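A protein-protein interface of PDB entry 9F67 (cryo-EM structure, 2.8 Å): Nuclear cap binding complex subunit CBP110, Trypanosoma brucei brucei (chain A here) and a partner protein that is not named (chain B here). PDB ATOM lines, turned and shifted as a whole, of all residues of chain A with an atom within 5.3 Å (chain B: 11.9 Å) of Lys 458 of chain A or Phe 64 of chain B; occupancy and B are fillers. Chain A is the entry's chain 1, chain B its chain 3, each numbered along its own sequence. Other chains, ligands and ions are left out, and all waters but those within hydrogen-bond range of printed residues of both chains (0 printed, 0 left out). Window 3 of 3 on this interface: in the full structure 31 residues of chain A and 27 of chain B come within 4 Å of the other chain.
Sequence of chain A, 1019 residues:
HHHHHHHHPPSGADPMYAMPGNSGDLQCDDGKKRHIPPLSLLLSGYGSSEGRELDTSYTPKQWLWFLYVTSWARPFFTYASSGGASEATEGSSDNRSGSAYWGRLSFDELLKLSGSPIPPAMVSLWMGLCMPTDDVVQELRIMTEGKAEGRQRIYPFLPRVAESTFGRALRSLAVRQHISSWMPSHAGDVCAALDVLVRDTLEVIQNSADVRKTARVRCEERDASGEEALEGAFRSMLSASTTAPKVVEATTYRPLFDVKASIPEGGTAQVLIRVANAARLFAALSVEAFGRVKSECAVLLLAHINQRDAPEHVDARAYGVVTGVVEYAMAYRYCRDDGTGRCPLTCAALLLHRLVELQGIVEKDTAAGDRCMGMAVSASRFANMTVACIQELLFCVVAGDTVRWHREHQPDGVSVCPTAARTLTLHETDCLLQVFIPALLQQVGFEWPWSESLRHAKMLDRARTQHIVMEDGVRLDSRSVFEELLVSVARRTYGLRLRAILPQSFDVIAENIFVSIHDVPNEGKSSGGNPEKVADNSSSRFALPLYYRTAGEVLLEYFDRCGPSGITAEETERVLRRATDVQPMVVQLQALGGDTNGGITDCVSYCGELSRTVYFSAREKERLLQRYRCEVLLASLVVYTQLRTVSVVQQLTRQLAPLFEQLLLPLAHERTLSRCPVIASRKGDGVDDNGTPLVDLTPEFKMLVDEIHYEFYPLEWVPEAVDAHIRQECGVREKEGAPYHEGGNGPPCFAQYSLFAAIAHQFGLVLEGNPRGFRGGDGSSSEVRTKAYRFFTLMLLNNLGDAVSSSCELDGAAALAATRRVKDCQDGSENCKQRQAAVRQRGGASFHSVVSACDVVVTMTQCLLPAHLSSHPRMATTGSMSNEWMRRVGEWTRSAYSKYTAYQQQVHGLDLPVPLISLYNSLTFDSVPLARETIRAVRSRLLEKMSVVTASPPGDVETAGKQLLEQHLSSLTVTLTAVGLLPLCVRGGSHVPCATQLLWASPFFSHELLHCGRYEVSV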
ATOM      1  N   VAL A 398       4.390  -0.802 -27.304  1.00  0.00           N
ATOM      2  CA  VAL A 398       5.098  -0.510 -26.060  1.00  0.00           C
ATOM      3  C   VAL A 398       6.258  -1.478 -25.850  1.00  0.00           C
ATOM      4  O   VAL A 398       7.368  -1.067 -25.497  1.00  0.00           O
ATOM      5  CB  VAL A 398       4.123  -0.534 -24.874  1.00  0.00           C
ATOM      6  CG1 VAL A 398       4.876  -0.390 -23.575  1.00  0.00           C
ATOM      7  CG2 VAL A 398       3.099   0.569 -25.016  1.00  0.00           C
ATOM      8  N   SER A 451      -6.809   2.156 -16.640  1.00  0.00           N
ATOM      9  CA  SER A 451      -5.877   1.807 -15.575  1.00  0.00           C
ATOM     10  C   SER A 451      -5.153   0.506 -15.883  1.00  0.00           C
ATOM     11  O   SER A 451      -3.932   0.408 -15.722  1.00  0.00           O
ATOM     12  CB  SER A 451      -6.619   1.709 -14.245  1.00  0.00           C
ATOM     13  OG  SER A 451      -7.886   1.099 -14.419  1.00  0.00           O
ATOM     14  N   SER A 453      -4.676  -0.963 -18.843  1.00  0.00           N
ATOM     15  CA  SER A 453      -3.782  -0.792 -19.980  1.00  0.00           C
ATOM     16  C   SER A 453      -2.512  -0.063 -19.575  1.00  0.00           C
ATOM     17  O   SER A 453      -1.411  -0.465 -19.963  1.00  0.00           O
ATOM     18  CB  SER A 453      -4.497  -0.044 -21.101  1.00  0.00           C
ATOM     19  OG  SER A 453      -5.258   1.034 -20.589  1.00  0.00           O
ATOM     20  N   LEU A 454      -2.641   1.009 -18.790  1.00  0.00           N
ATOM     21  CA  LEU A 454      -1.455   1.749 -18.376  1.00  0.00           C
ATOM     22  C   LEU A 454      -0.561   0.908 -17.479  1.00  0.00           C
ATOM     23  O   LEU A 454       0.667   0.931 -17.622  1.00  0.00           O
ATOM     24  CB  LEU A 454      -1.853   3.040 -17.668  1.00  0.00           C
ATOM     25  CG  LEU A 454      -0.682   3.980 -17.401  1.00  0.00           C
ATOM     26  CD1 LEU A 454       0.000   4.339 -18.701  1.00  0.00           C
ATOM     27  CD2 LEU A 454      -1.150   5.225 -16.681  1.00  0.00           C
ATOM     28  N   ARG A 455      -1.169   0.128 -16.583  1.00  0.00           N
ATOM     29  CA  ARG A 455      -0.339  -0.648 -15.624  1.00  0.00           C
ATOM     30  C   ARG A 455       0.471  -1.687 -16.408  1.00  0.00           C
ATOM     31  O   ARG A 455       1.703  -1.741 -16.219  1.00  0.00           O
ATOM     32  CB  ARG A 455      -1.205  -1.320 -14.555  1.00  0.00           C
ATOM     33  CG  ARG A 455      -0.384  -1.933 -13.432  1.00  0.00           C
ATOM     34  CD  ARG A 455      -1.181  -2.669 -12.373  1.00  0.00           C
ATOM     35  NE  ARG A 455      -1.873  -3.863 -12.841  1.00  0.00           N
ATOM     36  CZ  ARG A 455      -1.289  -4.937 -13.364  1.00  0.00           C
ATOM     37  NH1 ARG A 455       0.024  -4.994 -13.510  1.00  0.00           N
ATOM     38  NH2 ARG A 455      -2.025  -5.975 -13.719  1.00  0.00           N
ATOM     39  N   HIS A 456      -0.195  -2.461 -17.271  1.00  0.00           N
ATOM     40  CA  HIS A 456       0.498  -3.528 -18.046  1.00  0.00           C
ATOM     41  C   HIS A 456       1.559  -2.924 -18.972  1.00  0.00           C
ATOM     42  O   HIS A 456       2.655  -3.509 -19.078  1.00  0.00           O
ATOM     43  CB  HIS A 456      -0.496  -4.398 -18.824  1.00  0.00           C
ATOM     44  CG  HIS A 456      -1.369  -5.242 -17.960  1.00  0.00           C
ATOM     45  ND1 HIS A 456      -1.342  -6.616 -18.046  1.00  0.00           N
ATOM     46  CD2 HIS A 456      -2.256  -4.949 -17.004  1.00  0.00           C
ATOM     47  CE1 HIS A 456      -2.196  -7.127 -17.172  1.00  0.00           C
ATOM     48  NE2 HIS A 456      -2.765  -6.130 -16.532  1.00  0.00           N
ATOM     49  N   ALA A 457       1.261  -1.788 -19.604  1.00  0.00           N
ATOM     50  CA  ALA A 457       2.216  -1.220 -20.583  1.00  0.00           C
ATOM     51  C   ALA A 457       3.530  -0.886 -19.869  1.00  0.00           C
ATOM     52  O   ALA A 457       4.600  -1.156 -20.439  1.00  0.00           O
ATOM     53  CB  ALA A 457       1.618   0.000 -21.239  1.00  0.00           C
ATOM     54  N   LYS A 458       3.444  -0.339 -18.655  1.00  0.00           N
ATOM     55  CA  LYS A 458       4.669   0.046 -17.909  1.00  0.00           C
ATOM     56  C   LYS A 458       5.464  -1.203 -17.518  1.00  0.00           C
ATOM     57  O   LYS A 458       6.639  -1.046 -17.136  1.00  0.00           O
ATOM     58  CB  LYS A 458       4.306   0.833 -16.648  1.00  0.00           C
ATOM     59  CG  LYS A 458       3.565   2.141 -16.879  1.00  0.00           C
ATOM     60  CD  LYS A 458       3.253   2.864 -15.590  1.00  0.00           C
ATOM     61  CE  LYS A 458       2.527   4.173 -15.804  1.00  0.00           C
ATOM     62  NZ  LYS A 458       3.313   5.103 -16.649  1.00  0.00           N
ATOM     63  N   MET A 459       4.862  -2.393 -17.608  1.00  0.00           N
ATOM     64  CA  MET A 459       5.570  -3.579 -17.129  1.00  0.00           C
ATOM     65  C   MET A 459       6.266  -4.095 -18.351  1.00  0.00           C
ATOM     66  O   MET A 459       7.285  -4.785 -18.221  1.00  0.00           O
ATOM     67  CB  MET A 459       4.629  -4.660 -16.638  1.00  0.00           C
ATOM     68  CG  MET A 459       4.336  -4.576 -15.176  1.00  0.00           C
ATOM     69  SD  MET A 459       3.199  -5.876 -14.708  1.00  0.00           S
ATOM     70  CE  MET A 459       2.294  -6.075 -16.241  1.00  0.00           C
ATOM     71  N   LEU A 460       5.703  -3.776 -19.489  1.00  0.00           N
ATOM     72  CA  LEU A 460       6.282  -4.172 -20.765  1.00  0.00           C
ATOM     73  C   LEU A 460       7.511  -3.311 -20.977  1.00  0.00           C
ATOM     74  O   LEU A 460       8.383  -3.720 -21.723  1.00  0.00           O
ATOM     75  CB  LEU A 460       5.176  -4.084 -21.808  1.00  0.00           C
ATOM     76  CG  LEU A 460       4.006  -5.034 -21.600  1.00  0.00           C
ATOM     77  CD1 LEU A 460       3.157  -5.099 -22.848  1.00  0.00           C
ATOM     78  CD2 LEU A 460       4.498  -6.420 -21.233  1.00  0.00           C
ATOM     79  N   ASP A 461       7.544  -2.144 -20.381  1.00  0.00           N
ATOM     80  CA  ASP A 461       8.659  -1.183 -20.537  1.00  0.00           C
ATOM     81  C   ASP A 461       9.962  -1.665 -19.951  1.00  0.00           C
ATOM     82  O   ASP A 461      10.998  -1.401 -20.541  1.00  0.00           O
ATOM     83  CB  ASP A 461       8.378   0.125 -19.828  1.00  0.00           C
ATOM     84  CG  ASP A 461       7.344   1.016 -20.476  1.00  0.00           C
ATOM     85  OD1 ASP A 461       6.819   0.629 -21.521  1.00  0.00           O
ATOM     86  OD2 ASP A 461       7.103   2.104 -19.936  1.00  0.00           O
ATOM     87  N   ARG A 462       9.916  -2.346 -18.843  1.00  0.00           N
ATOM     88  CA  ARG A 462      11.117  -2.715 -18.083  1.00  0.00           C
ATOM     89  C   ARG A 462      12.012  -3.597 -18.912  1.00  0.00           C
ATOM     90  O   ARG A 462      13.211  -3.624 -18.666  1.00  0.00           O
ATOM     91  CB  ARG A 462      10.660  -3.481 -16.855  1.00  0.00           C
ATOM     92  CG  ARG A 462       9.757  -2.674 -15.937  1.00  0.00           C
ATOM     93  CD  ARG A 462       9.169  -3.512 -14.821  1.00  0.00           C
ATOM     94  NE  ARG A 462       8.301  -4.540 -15.377  1.00  0.00           N
ATOM     95  CZ  ARG A 462       8.473  -5.847 -15.222  1.00  0.00           C
ATOM     96  NH1 ARG A 462       7.626  -6.693 -15.780  1.00  0.00           N
ATOM     97  NH2 ARG A 462       9.493  -6.304 -14.517  1.00  0.00           N
ATOM     98  N   SER A 478       5.651   3.654 -22.527  1.00  0.00           N
ATOM     99  CA  SER A 478       4.228   3.715 -22.215  1.00  0.00           C
ATOM    100  C   SER A 478       3.757   5.154 -22.085  1.00  0.00           C
ATOM    101  O   SER A 478       2.679   5.515 -22.580  1.00  0.00           O
ATOM    102  CB  SER A 478       3.942   2.946 -20.931  1.00  0.00           C
ATOM    103  OG  SER A 478       4.916   3.234 -19.947  1.00  0.00           O
ATOM    104  N   ARG A 479       4.553   5.989 -21.418  1.00  0.00           N
ATOM    105  CA  ARG A 479       4.188   7.386 -21.235  1.00  0.00           C
ATOM    106  C   ARG A 479       4.019   8.082 -22.574  1.00  0.00           C
ATOM    107  O   ARG A 479       3.050   8.817 -22.785  1.00  0.00           O
ATOM    108  CB  ARG A 479       5.248   8.091 -20.392  1.00  0.00           C
ATOM    109  CG  ARG A 479       4.889   9.503 -19.987  1.00  0.00           C
ATOM    110  CD  ARG A 479       6.129  10.273 -19.575  1.00  0.00           C
ATOM    111  NE  ARG A 479       5.881  11.174 -18.457  1.00  0.00           N
ATOM    112  CZ  ARG A 479       5.224  12.321 -18.544  1.00  0.00           C
ATOM    113  NH1 ARG A 479       4.726  12.749 -19.692  1.00  0.00           N
ATOM    114  NH2 ARG A 479       5.066  13.062 -17.452  1.00  0.00           N
ATOM    115  N   SER A 505      -4.281   7.479 -11.796  1.00  0.00           N
ATOM    116  CA  SER A 505      -2.956   7.075 -12.237  1.00  0.00           C
ATOM    117  C   SER A 505      -2.494   7.831 -13.471  1.00  0.00           C
ATOM    118  O   SER A 505      -1.312   7.756 -13.819  1.00  0.00           O
ATOM    119  CB  SER A 505      -2.930   5.575 -12.518  1.00  0.00           C
ATOM    120  OG  SER A 505      -3.083   5.314 -13.901  1.00  0.00           O
ATOM    121  N   ILE A 509       0.355  12.233 -16.730  1.00  0.00           N
ATOM    122  CA  ILE A 509       0.139  12.380 -18.166  1.00  0.00           C
ATOM    123  C   ILE A 509      -0.873  13.483 -18.445  1.00  0.00           C
ATOM    124  O   ILE A 509      -0.669  14.329 -19.325  1.00  0.00           O
ATOM    125  CB  ILE A 509      -0.308  11.040 -18.776  1.00  0.00           C
ATOM    126  CG1 ILE A 509       0.873  10.087 -18.904  1.00  0.00           C
ATOM    127  CG2 ILE A 509      -0.946  11.258 -20.134  1.00  0.00           C
ATOM    128  CD1 ILE A 509       0.465   8.652 -19.061  1.00  0.00           C
ATOM    129  N   THR B  56     -11.105  -7.122 -19.092  1.00  0.00           N
ATOM    130  CA  THR B  56     -10.300  -6.948 -17.890  1.00  0.00           C
ATOM    131  C   THR B  56     -10.369  -8.174 -16.986  1.00  0.00           C
ATOM    132  O   THR B  56      -9.349  -8.594 -16.428  1.00  0.00           O
ATOM    133  CB  THR B  56     -10.758  -5.700 -17.139  1.00  0.00           C
ATOM    134  OG1 THR B  56     -10.483  -4.541 -17.933  1.00  0.00           O
ATOM    135  CG2 THR B  56     -10.039  -5.575 -15.805  1.00  0.00           C
ATOM    136  N   GLY B  60      -6.699 -11.559 -17.309  1.00  0.00           N
ATOM    137  CA  GLY B  60      -5.938 -11.270 -16.110  1.00  0.00           C
ATOM    138  C   GLY B  60      -5.365  -9.875 -15.984  1.00  0.00           C
ATOM    139  O   GLY B  60      -4.187  -9.718 -15.651  1.00  0.00           O
ATOM    140  N   LEU B  61      -6.172  -8.855 -16.245  1.00  0.00           N
ATOM    141  CA  LEU B  61      -5.735  -7.472 -16.125  1.00  0.00           C
ATOM    142  C   LEU B  61      -6.294  -6.874 -14.843  1.00  0.00           C
ATOM    143  O   LEU B  61      -7.484  -7.032 -14.548  1.00  0.00           O
ATOM    144  CB  LEU B  61      -6.179  -6.649 -17.333  1.00  0.00           C
ATOM    145  CG  LEU B  61      -5.495  -6.972 -18.661  1.00  0.00           C
ATOM    146  CD1 LEU B  61      -6.419  -7.788 -19.541  1.00  0.00           C
ATOM    147  CD2 LEU B  61      -5.065  -5.704 -19.367  1.00  0.00           C
ATOM    148  N   THR B  62      -5.438  -6.199 -14.082  1.00  0.00           N
ATOM    149  CA  THR B  62      -5.820  -5.592 -12.815  1.00  0.00           C
ATOM    150  C   THR B  62      -5.462  -4.115 -12.826  1.00  0.00           C
ATOM    151  O   THR B  62      -4.470  -3.704 -13.433  1.00  0.00           O
ATOM    152  CB  THR B  62      -5.131  -6.279 -11.633  1.00  0.00           C
ATOM    153  OG1 THR B  62      -3.710  -6.214 -11.804  1.00  0.00           O
ATOM    154  CG2 THR B  62      -5.554  -7.732 -11.538  1.00  0.00           C
ATOM    155  N   LYS B  63      -6.278  -3.318 -12.146  1.00  0.00           N
ATOM    156  CA  LYS B  63      -6.053  -1.885 -12.079  1.00  0.00           C
ATOM    157  C   LYS B  63      -4.874  -1.570 -11.164  1.00  0.00           C
ATOM    158  O   LYS B  63      -4.338  -2.436 -10.470  1.00  0.00           O
ATOM    159  CB  LYS B  63      -7.312  -1.165 -11.602  1.00  0.00           C
ATOM    160  CG  LYS B  63      -8.536  -1.456 -12.437  1.00  0.00           C
ATOM    161  CD  LYS B  63      -9.814  -1.239 -11.658  1.00  0.00           C
ATOM    162  CE  LYS B  63     -10.128   0.234 -11.519  1.00  0.00           C
ATOM    163  NZ  LYS B  63     -10.928   0.734 -12.666  1.00  0.00           N
ATOM    164  N   PHE B  64      -4.467  -0.304 -11.178  1.00  0.00           N
ATOM    165  CA  PHE B  64      -3.356   0.134 -10.349  1.00  0.00           C
ATOM    166  C   PHE B  64      -3.703   0.005  -8.873  1.00  0.00           C
ATOM    167  O   PHE B  64      -4.845   0.216  -8.458  1.00  0.00           O
ATOM    168  CB  PHE B  64      -3.001   1.587 -10.655  1.00  0.00           C
ATOM    169  CG  PHE B  64      -1.836   1.750 -11.580  1.00  0.00           C
ATOM    170  CD1 PHE B  64      -0.550   1.507 -11.143  1.00  0.00           C
ATOM    171  CD2 PHE B  64      -2.025   2.170 -12.881  1.00  0.00           C
ATOM    172  CE1 PHE B  64       0.519   1.663 -11.988  1.00  0.00           C
ATOM    173  CE2 PHE B  64      -0.959   2.331 -13.728  1.00  0.00           C
ATOM    174  CZ  PHE B  64       0.316   2.077 -13.282  1.00  0.00           C
ATOM    175  N   ALA B  65      -2.701  -0.348  -8.074  1.00  0.00           N
ATOM    176  CA  ALA B  65      -2.854  -0.276  -6.629  1.00  0.00           C
ATOM    177  C   ALA B  65      -2.815   1.188  -6.222  1.00  0.00           C
ATOM    178  O   ALA B  65      -1.739   1.753  -6.002  1.00  0.00           O
ATOM    179  CB  ALA B  65      -1.762  -1.075  -5.919  1.00  0.00           C
ATOM    180  N   GLY B  66      -3.984   1.807  -6.123  1.00  0.00           N
ATOM    181  CA  GLY B  66      -4.084   3.242  -5.956  1.00  0.00           C
ATOM    182  C   GLY B  66      -5.263   3.770  -6.741  1.00  0.00           C
ATOM    183  O   GLY B  66      -5.851   4.797  -6.392  1.00  0.00           O
ATOM    184  N   ASP B  67      -5.666   3.060  -7.762  1.00  0.00           N
ATOM    185  CA  ASP B  67      -6.905   3.423  -8.452  1.00  0.00           C
ATOM    186  C   ASP B  67      -7.913   2.490  -7.822  1.00  0.00           C
ATOM    187  O   ASP B  67      -9.090   2.848  -7.798  1.00  0.00           O
ATOM    188  CB  ASP B  67      -6.813   3.236  -9.955  1.00  0.00           C
ATOM    189  CG  ASP B  67      -5.830   4.125 -10.686  1.00  0.00           C
ATOM    190  OD1 ASP B  67      -5.968   5.353 -10.589  1.00  0.00           O
ATOM    191  OD2 ASP B  67      -5.033   3.581 -11.450  1.00  0.00           O
ATOM    192  N   ILE B  68      -7.457   1.325  -7.363  1.00  0.00           N
ATOM    193  CA  ILE B  68      -8.329   0.359  -6.643  1.00  0.00           C
ATOM    194  C   ILE B  68      -8.753   1.009  -5.339  1.00  0.00           C
ATOM    195  O   ILE B  68      -9.915   0.855  -4.979  1.00  0.00           O
ATOM    196  CB  ILE B  68      -7.670  -1.008  -6.504  1.00  0.00           C
ATOM    197  CG1 ILE B  68      -7.369  -1.612  -7.873  1.00  0.00           C
ATOM    198  CG2 ILE B  68      -8.537  -1.943  -5.683  1.00  0.00           C
ATOM    199  CD1 ILE B  68      -6.724  -2.972  -7.811  1.00  0.00           C
ATOM    200  N   GLU B  69      -7.874   1.769  -4.708  1.00  0.00           N
ATOM    201  CA  GLU B  69      -8.175   2.438  -3.417  1.00  0.00           C
ATOM    202  C   GLU B  69      -9.076   3.642  -3.622  1.00  0.00           C
ATOM    203  O   GLU B  69      -9.348   4.315  -2.650  1.00  0.00           O
ATOM    204  CB  GLU B  69      -6.944   2.789  -2.597  1.00  0.00           C
ATOM    205  CG  GLU B  69      -6.130   1.569  -2.235  1.00  0.00           C
ATOM    206  CD  GLU B  69      -6.917   0.535  -1.450  1.00  0.00           C
ATOM    207  OE1 GLU B  69      -7.402   0.871  -0.353  1.00  0.00           O
ATOM    208  OE2 GLU B  69      -7.051  -0.602  -1.945  1.00  0.00           O
ATOM    209  N   ALA B  70      -9.437   3.970  -4.839  1.00  0.00           N
ATOM    210  CA  ALA B  70     -10.478   4.969  -4.969  1.00  0.00           C
ATOM    211  C   ALA B  70     -11.762   4.172  -4.728  1.00  0.00           C
ATOM    212  O   ALA B  70     -12.522   3.945  -5.689  1.00  0.00           O
ATOM    213  CB  ALA B  70     -10.431   5.560  -6.311  1.00  0.00           C
ATOM    214  N   GLU B  71     -11.912   3.613  -3.508  1.00  0.00           N
ATOM    215  CA  GLU B  71     -13.125   2.927  -3.002  1.00  0.00           C
ATOM    216  C   GLU B  71     -13.638   3.909  -1.969  1.00  0.00           C
ATOM    217  O   GLU B  71     -14.608   3.605  -1.288  1.00  0.00           O
ATOM    218  CB  GLU B  71     -12.670   1.652  -2.332  1.00  0.00           C
ATOM    219  CG  GLU B  71     -11.718   1.880  -1.186  1.00  0.00           C
ATOM    220  CD  GLU B  71     -11.242   0.586  -0.558  1.00  0.00           C
ATOM    221  OE1 GLU B  71     -11.661  -0.480  -1.036  1.00  0.00           O
ATOM    222  OE2 GLU B  71     -10.463   0.648   0.408  1.00  0.00           O
ATOM    223  N   ARG B  72     -12.919   5.031  -1.841  1.00  0.00           N
ATOM    224  CA  ARG B  72     -13.331   6.125  -0.928  1.00  0.00           C
ATOM    225  C   ARG B  72     -13.951   7.189  -1.833  1.00  0.00           C
ATOM    226  O   ARG B  72     -13.855   8.383  -1.485  1.00  0.00           O
ATOM    227  CB  ARG B  72     -12.104   6.638  -0.172  1.00  0.00           C
ATOM    228  CG  ARG B  72     -11.377   5.549   0.603  1.00  0.00           C
ATOM    229  CD  ARG B  72     -10.138   6.045   1.317  1.00  0.00           C
ATOM    230  NE  ARG B  72      -9.467   4.964   2.026  1.00  0.00           N
ATOM    231  CZ  ARG B  72      -8.356   5.106   2.737  1.00  0.00           C
ATOM    232  NH1 ARG B  72      -7.783   6.293   2.838  1.00  0.00           N
ATOM    233  NH2 ARG B  72      -7.821   4.061   3.344  1.00  0.00           N
ATOM    234  N   GLY B  74     -13.236   8.362  -5.168  1.00  0.00           N
ATOM    235  CA  GLY B  74     -12.559   9.324  -6.028  1.00  0.00           C
ATOM    236  C   GLY B  74     -12.392   8.756  -7.412  1.00  0.00           C
ATOM    237  O   GLY B  74     -11.562   9.298  -8.152  1.00  0.00           O
ATOM    238  N   GLU B  75     -13.118   7.720  -7.773  1.00  0.00           N
ATOM    239  CA  GLU B  75     -12.823   6.970  -9.028  1.00  0.00           C
ATOM    240  C   GLU B  75     -13.438   7.630 -10.248  1.00  0.00           C
ATOM    241  O   GLU B  75     -14.186   8.559 -10.056  1.00  0.00           O
ATOM    242  CB  GLU B  75     -13.234   5.510  -8.792  1.00  0.00           C
ATOM    243  CG  GLU B  75     -12.842   4.537  -9.891  1.00  0.00           C
ATOM    244  CD  GLU B  75     -13.097   3.076  -9.564  1.00  0.00           C
ATOM    245  OE1 GLU B  75     -13.583   2.792  -8.448  1.00  0.00           O
ATOM    246  OE2 GLU B  75     -12.809   2.223 -10.426  1.00  0.00           O
ATOM    247  N   GLY B  76     -13.163   7.137 -11.447  1.00  0.00           N
ATOM    248  CA  GLY B  76     -13.828   7.825 -12.541  1.00  0.00           C
ATOM    249  C   GLY B  76     -15.332   7.902 -12.366  1.00  0.00           C
ATOM    250  O   GLY B  76     -15.929   6.887 -12.061  1.00  0.00           O
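The guanidinium group (NH2) of Arg 455 of chain A lies within hydrogen-bond range of the side-chain hydroxyl (OG1) of Thr 62 of chain B (2.6 Å).
The backbone NH of Ser 505 of chain A is in hydrogen-bond range of the side-chain carboxylate of Asp 67 of chain B.
The backbone carbonyl oxygen (O) of Thr 56 of chain B sits at hydrogen-bond distance from the backbone NH (N) of Leu 61 of chain B (3.2 Å).
NH2 of Arg 455 of chain A is in hydrogen-bond range of NE2 of His 456 of chain A, at 2.9 Å.
NH1 of Arg 455 of chain A lies within hydrogen-bond range of SD of Met 459 of chain A.
NZ of Lys 63 of chain B is in salt-bridge range of OE2 of Glu 75 of chain B (3.3 Å).
Among the printed residues, pairs that only touch across the chains: Ser 451 of chain A with Lys 63 of chain B (3.3 Å), Ser 451 of chain A with Phe 64 of chain B (3.8 Å), Ser 451 of chain A with Asp 67 of chain B (3.7 Å), Arg 455 of chain A with Lys 63 of chain B (3.7 Å), Arg 455 of chain A with Phe 64 of chain B (3.6 Å), His 456 of chain A with Gly 60 of chain B (3.6 Å), His 456 of chain A with Leu 61 of chain B (3.3 Å), His 456 of chain A with Thr 62 of chain B (3.6 Å), Lys 458 of chain A with Phe 64 of chain B (3.8 Å) and Ser 505 of chain A with Phe 64 of chain B (3.5 Å).
Printed residues of chain B within 4 Å of His 456 of chain A: Gly 60, Leu 61 and Thr 62.
No residue of chain B comes within 4 Å of Ala 457 of chain A.
Of chain B, only Phe 64 comes within 4 Å of Lys 458 of chain A.
No residue of chain B comes within 4 Å of Met 459 of chain A.
No residue of chain B comes within 4 Å of Leu 460 of chain A.
No residue of chain B comes within 4 Å of Asp 461 of chain A.
No residue of chain B comes within 4 Å of Arg 462 of chain A.
Ser 505 of chain A touches two residues of chain B.
Of the printed residues of chain A, Leu 61 of chain B touches His 456 (3.3 Å).
Printed residues of chain A within 4 Å of Thr 62 of chain B: Arg 455 (2.6 Å) and His 456 (3.6 Å).
Of the printed residues of chain A, Lys 63 of chain B touches Ser 451 and Arg 455.
Of chain A, only Ser 451, Arg 455, Lys 458 and Ser 505 come within 4 Å of Phe 64 of chain B.
Printed residues of chain A within 4 Å of Asp 67 of chain B: Ser 451 and Ser 505.
Ala 70 of chain B touches none of the printed residues of chain A.
The nearest residue of chain B that does not touch Lys 458 of chain A is Asp 67 of chain B (8.7 Å).
The nearest residue of chain A that does not touch Phe 64 of chain B is Leu 454 of chain A (4.03 Å).
The nearest printed residue of chain A that does not touch Leu 61 of chain B is Arg 455 of chain A (4.5 Å).
Of the 17 printed residues of chain B, 6 touch a printed residue of chain A.
Along chain B the printed residues that touch a printed residue of chain A span positions 60 to 67.
Printed residues of chain A that touch a printed residue of chain B: Ser 451, Arg 455, His 456, Lys 458 and Ser 505.
Hydrophobic or aromatic side chains of chain A that line the printed part of chain B: His 456.
Along chain A the printed residues that touch a printed residue of chain B span positions 451 to 505.
Among the printed residues, 12 pairs touch across the chains.
Among the printed residues, no Asp or Glu carboxylate lies within 4 Å of a Lys or Arg side-chain nitrogen of the other chain.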
